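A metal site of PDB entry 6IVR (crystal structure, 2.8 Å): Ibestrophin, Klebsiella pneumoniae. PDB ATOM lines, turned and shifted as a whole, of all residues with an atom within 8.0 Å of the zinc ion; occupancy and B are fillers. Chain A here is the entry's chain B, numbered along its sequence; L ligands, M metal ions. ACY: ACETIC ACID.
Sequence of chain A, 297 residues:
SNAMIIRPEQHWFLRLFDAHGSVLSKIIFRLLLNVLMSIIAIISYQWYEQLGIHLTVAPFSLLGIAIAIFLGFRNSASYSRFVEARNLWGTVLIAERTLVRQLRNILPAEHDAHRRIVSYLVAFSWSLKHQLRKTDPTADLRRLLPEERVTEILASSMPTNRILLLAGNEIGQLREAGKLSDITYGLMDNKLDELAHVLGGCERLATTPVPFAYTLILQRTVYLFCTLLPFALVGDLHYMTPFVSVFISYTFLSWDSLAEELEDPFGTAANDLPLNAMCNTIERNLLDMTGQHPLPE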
ATOM      1  N   VAL A 100      16.962 -24.894 -22.956  1.00  0.00           N
ATOM      2  CA  VAL A 100      16.393 -24.215 -21.791  1.00  0.00           C
ATOM      3  C   VAL A 100      17.042 -24.694 -20.503  1.00  0.00           C
ATOM      4  O   VAL A 100      17.267 -23.897 -19.579  1.00  0.00           O
ATOM      5  CB  VAL A 100      14.863 -24.413 -21.770  1.00  0.00           C
ATOM      6  CG1 VAL A 100      14.286 -24.012 -20.424  1.00  0.00           C
ATOM      7  CG2 VAL A 100      14.265 -23.577 -22.870  1.00  0.00           C
ATOM      8  N   LEU A 103      20.332 -22.964 -20.023  1.00  0.00           N
ATOM      9  CA  LEU A 103      20.140 -21.593 -19.596  1.00  0.00           C
ATOM     10  C   LEU A 103      19.794 -21.521 -18.119  1.00  0.00           C
ATOM     11  O   LEU A 103      20.366 -20.737 -17.369  1.00  0.00           O
ATOM     12  CB  LEU A 103      19.061 -20.926 -20.438  1.00  0.00           C
ATOM     13  CG  LEU A 103      19.479 -20.453 -21.816  1.00  0.00           C
ATOM     14  CD1 LEU A 103      18.212 -20.090 -22.583  1.00  0.00           C
ATOM     15  CD2 LEU A 103      20.424 -19.265 -21.740  1.00  0.00           C
ATOM     16  N   ARG A 104      18.845 -22.366 -17.686  1.00  0.00           N
ATOM     17  CA  ARG A 104      18.539 -22.461 -16.266  1.00  0.00           C
ATOM     18  C   ARG A 104      19.764 -22.915 -15.457  1.00  0.00           C
ATOM     19  O   ARG A 104      19.967 -22.458 -14.325  1.00  0.00           O
ATOM     20  CB  ARG A 104      17.314 -23.382 -16.056  1.00  0.00           C
ATOM     21  CG  ARG A 104      15.961 -22.710 -16.422  1.00  0.00           C
ATOM     22  CD  ARG A 104      14.731 -23.636 -16.552  1.00  0.00           C
ATOM     23  NE  ARG A 104      13.510 -22.858 -16.866  1.00  0.00           N
ATOM     24  CZ  ARG A 104      12.289 -23.345 -17.150  1.00  0.00           C
ATOM     25  NH1 ARG A 104      11.294 -22.505 -17.417  1.00  0.00           N
ATOM     26  NH2 ARG A 104      12.041 -24.649 -17.212  1.00  0.00           N
ATOM     27  N   LEU A 107      22.976 -19.746 -16.414  1.00  0.00           N
ATOM     28  CA  LEU A 107      22.536 -18.400 -16.068  1.00  0.00           C
ATOM     29  C   LEU A 107      21.209 -18.488 -15.341  1.00  0.00           C
ATOM     30  O   LEU A 107      20.184 -18.048 -15.877  1.00  0.00           O
ATOM     31  CB  LEU A 107      22.442 -17.502 -17.298  1.00  0.00           C
ATOM     32  CG  LEU A 107      23.609 -17.536 -18.258  1.00  0.00           C
ATOM     33  CD1 LEU A 107      23.300 -16.836 -19.592  1.00  0.00           C
ATOM     34  CD2 LEU A 107      24.799 -16.887 -17.539  1.00  0.00           C
ATOM     35  N   PRO A 108      21.180 -19.041 -14.131  1.00  0.00           N
ATOM     36  CA  PRO A 108      19.892 -19.309 -13.472  1.00  0.00           C
ATOM     37  C   PRO A 108      19.064 -18.071 -13.181  1.00  0.00           C
ATOM     38  O   PRO A 108      17.842 -18.187 -13.057  1.00  0.00           O
ATOM     39  CB  PRO A 108      20.296 -20.006 -12.169  1.00  0.00           C
ATOM     40  CG  PRO A 108      21.686 -19.669 -11.980  1.00  0.00           C
ATOM     41  CD  PRO A 108      22.301 -19.531 -13.323  1.00  0.00           C
ATOM     42  N   ALA A 109      19.693 -16.900 -13.055  1.00  0.00           N
ATOM     43  CA  ALA A 109      18.974 -15.685 -12.678  1.00  0.00           C
ATOM     44  C   ALA A 109      18.474 -14.888 -13.866  1.00  0.00           C
ATOM     45  O   ALA A 109      17.591 -14.037 -13.704  1.00  0.00           O
ATOM     46  CB  ALA A 109      19.874 -14.795 -11.817  1.00  0.00           C
ATOM     47  N   GLU A 110      19.005 -15.172 -15.057  1.00  0.00           N
ATOM     48  CA  GLU A 110      18.758 -14.372 -16.261  1.00  0.00           C
ATOM     49  C   GLU A 110      17.374 -14.640 -16.857  1.00  0.00           C
ATOM     50  O   GLU A 110      17.237 -15.012 -18.017  1.00  0.00           O
ATOM     51  CB  GLU A 110      19.848 -14.686 -17.262  1.00  0.00           C
ATOM     52  CG  GLU A 110      21.164 -14.078 -16.916  1.00  0.00           C
ATOM     53  CD  GLU A 110      21.170 -12.573 -17.171  1.00  0.00           C
ATOM     54  OE1 GLU A 110      20.229 -12.054 -17.832  1.00  0.00           O
ATOM     55  OE2 GLU A 110      22.142 -11.921 -16.721  1.00  0.00           O
ATOM     56  N   HIS A 111      16.337 -14.401 -16.050  1.00  0.00           N
ATOM     57  CA  HIS A 111      14.992 -14.820 -16.444  1.00  0.00           C
ATOM     58  C   HIS A 111      14.451 -14.030 -17.623  1.00  0.00           C
ATOM     59  O   HIS A 111      13.630 -14.539 -18.393  1.00  0.00           O
ATOM     60  CB  HIS A 111      14.035 -14.699 -15.255  1.00  0.00           C
ATOM     61  CG  HIS A 111      14.429 -15.545 -14.088  1.00  0.00           C
ATOM     62  ND1 HIS A 111      14.428 -16.924 -14.121  1.00  0.00           N
ATOM     63  CD2 HIS A 111      14.838 -15.203 -12.840  1.00  0.00           C
ATOM     64  CE1 HIS A 111      14.830 -17.395 -12.951  1.00  0.00           C
ATOM     65  NE2 HIS A 111      15.076 -16.361 -12.153  1.00  0.00           N
ATOM     66  N   ASP A 112      14.849 -12.761 -17.785  1.00  0.00           N
ATOM     67  CA  ASP A 112      14.379 -12.034 -18.956  1.00  0.00           C
ATOM     68  C   ASP A 112      14.908 -12.690 -20.223  1.00  0.00           C
ATOM     69  O   ASP A 112      14.188 -12.808 -21.225  1.00  0.00           O
ATOM     70  CB  ASP A 112      14.783 -10.558 -18.882  1.00  0.00           C
ATOM     71  CG  ASP A 112      13.931  -9.749 -17.876  1.00  0.00           C
ATOM     72  OD1 ASP A 112      12.708  -9.603 -18.097  1.00  0.00           O
ATOM     73  OD2 ASP A 112      14.496  -9.274 -16.856  1.00  0.00           O
ATOM     74  N   ALA A 113      16.150 -13.170 -20.184  1.00  0.00           N
ATOM     75  CA  ALA A 113      16.721 -13.920 -21.295  1.00  0.00           C
ATOM     76  C   ALA A 113      16.033 -15.273 -21.467  1.00  0.00           C
ATOM     77  O   ALA A 113      15.668 -15.639 -22.594  1.00  0.00           O
ATOM     78  CB  ALA A 113      18.232 -14.100 -21.091  1.00  0.00           C
ATOM     79  N   HIS A 114      15.848 -16.029 -20.365  1.00  0.00           N
ATOM     80  CA  HIS A 114      15.079 -17.270 -20.446  1.00  0.00           C
ATOM     81  C   HIS A 114      13.776 -17.076 -21.180  1.00  0.00           C
ATOM     82  O   HIS A 114      13.456 -17.806 -22.116  1.00  0.00           O
ATOM     83  CB  HIS A 114      14.780 -17.815 -19.050  1.00  0.00           C
ATOM     84  CG  HIS A 114      15.982 -18.079 -18.228  1.00  0.00           C
ATOM     85  ND1 HIS A 114      15.939 -18.144 -16.854  1.00  0.00           N
ATOM     86  CD2 HIS A 114      17.274 -18.298 -18.575  1.00  0.00           C
ATOM     87  CE1 HIS A 114      17.156 -18.380 -16.393  1.00  0.00           C
ATOM     88  NE2 HIS A 114      17.984 -18.484 -17.416  1.00  0.00           N
ATOM     89  N   ARG A 115      13.015 -16.061 -20.752  1.00  0.00           N
ATOM     90  CA  ARG A 115      11.693 -15.782 -21.329  1.00  0.00           C
ATOM     91  C   ARG A 115      11.817 -15.438 -22.818  1.00  0.00           C
ATOM     92  O   ARG A 115      11.084 -15.990 -23.652  1.00  0.00           O
ATOM     93  CB  ARG A 115      11.045 -14.640 -20.543  1.00  0.00           C
ATOM     94  CG  ARG A 115       9.624 -14.252 -20.911  1.00  0.00           C
ATOM     95  CD  ARG A 115       8.994 -13.326 -19.831  1.00  0.00           C
ATOM     96  NE  ARG A 115       9.942 -12.400 -19.194  1.00  0.00           N
ATOM     97  CZ  ARG A 115      10.377 -12.481 -17.931  1.00  0.00           C
ATOM     98  NH1 ARG A 115       9.973 -13.456 -17.110  1.00  0.00           N
ATOM     99  NH2 ARG A 115      11.231 -11.572 -17.480  1.00  0.00           N
ATOM    100  N   VAL A 118      12.874 -18.749 -24.848  1.00  0.00           N
ATOM    101  CA  VAL A 118      11.791 -19.716 -24.943  1.00  0.00           C
ATOM    102  C   VAL A 118      10.750 -19.286 -25.972  1.00  0.00           C
ATOM    103  O   VAL A 118      10.248 -20.098 -26.762  1.00  0.00           O
ATOM    104  CB  VAL A 118      11.155 -19.948 -23.564  1.00  0.00           C
ATOM    105  CG1 VAL A 118       9.787 -20.631 -23.731  1.00  0.00           C
ATOM    106  CG2 VAL A 118      12.071 -20.780 -22.691  1.00  0.00           C
ATOM    107  N   THR A 290       4.746 -21.355 -15.642  1.00  0.00           N
ATOM    108  CA  THR A 290       5.114 -19.961 -15.909  1.00  0.00           C
ATOM    109  C   THR A 290       6.575 -19.840 -16.354  1.00  0.00           C
ATOM    110  O   THR A 290       7.117 -18.734 -16.483  1.00  0.00           O
ATOM    111  CB  THR A 290       4.757 -19.073 -14.678  1.00  0.00           C
ATOM    112  OG1 THR A 290       3.349 -18.771 -14.708  1.00  0.00           O
ATOM    113  CG2 THR A 290       5.520 -17.728 -14.576  1.00  0.00           C
ATOM    114  N   GLY A 291       7.215 -20.958 -16.673  1.00  0.00           N
ATOM    115  CA  GLY A 291       8.630 -20.929 -16.962  1.00  0.00           C
ATOM    116  C   GLY A 291       9.448 -20.804 -15.694  1.00  0.00           C
ATOM    117  O   GLY A 291      10.575 -20.295 -15.737  1.00  0.00           O
ATOM    118  N   GLN A 292       8.918 -21.262 -14.557  1.00  0.00           N
ATOM    119  CA  GLN A 292       9.619 -21.176 -13.286  1.00  0.00           C
ATOM    120  C   GLN A 292      10.251 -22.515 -12.924  1.00  0.00           C
ATOM    121  O   GLN A 292       9.641 -23.580 -13.116  1.00  0.00           O
ATOM    122  CB  GLN A 292       8.686 -20.683 -12.159  1.00  0.00           C
ATOM    123  CG  GLN A 292       9.373 -20.165 -10.843  1.00  0.00           C
ATOM    124  CD  GLN A 292      10.691 -19.384 -11.036  1.00  0.00           C
ATOM    125  OE1 GLN A 292      11.757 -19.952 -11.284  1.00  0.00           O
ATOM    126  NE2 GLN A 292      10.606 -18.062 -10.938  1.00  0.00           N
ATOM    127  N   HIS A 293      11.459 -22.432 -12.378  1.00  0.00           N
ATOM    128  CA  HIS A 293      12.378 -23.530 -12.160  1.00  0.00           C
ATOM    129  C   HIS A 293      13.007 -23.397 -10.776  1.00  0.00           C
ATOM    130  O   HIS A 293      12.999 -22.307 -10.193  1.00  0.00           O
ATOM    131  CB  HIS A 293      13.477 -23.535 -13.246  1.00  0.00           C
ATOM    132  CG  HIS A 293      13.977 -22.171 -13.638  1.00  0.00           C
ATOM    133  ND1 HIS A 293      15.252 -21.734 -13.351  1.00  0.00           N
ATOM    134  CD2 HIS A 293      13.373 -21.155 -14.307  1.00  0.00           C
ATOM    135  CE1 HIS A 293      15.414 -20.502 -13.823  1.00  0.00           C
ATOM    136  NE2 HIS A 293      14.288 -20.129 -14.405  1.00  0.00           N
HETATM  137  C   ACY L   1      12.132 -18.115 -16.980  1.00  0.00           C
HETATM  138  O   ACY L   1      12.715 -17.385 -16.186  1.00  0.00           O
HETATM  139  OXT ACY L   1      12.493 -19.317 -17.305  1.00  0.00           O
HETATM  140  CH3 ACY L   1      10.839 -17.635 -17.740  1.00  0.00           C
HETATM  141 ZN    ZN M   1      14.357 -18.460 -15.616  1.00  0.00          ZN
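The backbone carbonyl oxygen (O) of Leu 103 is in hydrogen-bond range of a ring nitrogen (NE2) of His 114 (3.3 Å). NE2 of His 114 lies within hydrogen-bond range of O of Leu 107 (2.7 Å). A ring nitrogen (NE2) of His 111 sits close to the backbone carbonyl oxygen (O) of Pro 108, 3.4 Å away.
The zinc ion is bound by a ring nitrogen (ND1) of His 114, an oxygen (O) of the ligand, a ring nitrogen (NE2) of His 293 and a ring nitrogen (ND1) of His 111. The zinc ion has four donor atoms within binding distance. Slightly farther from the zinc ion lies OXT of the ligand (2.7 Å).
Of the 17 residues printed, 3 come within 4 Å of the zinc ion. The nearest printed residue that does not touch the zinc ion is Gly 291 (4.2 Å).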
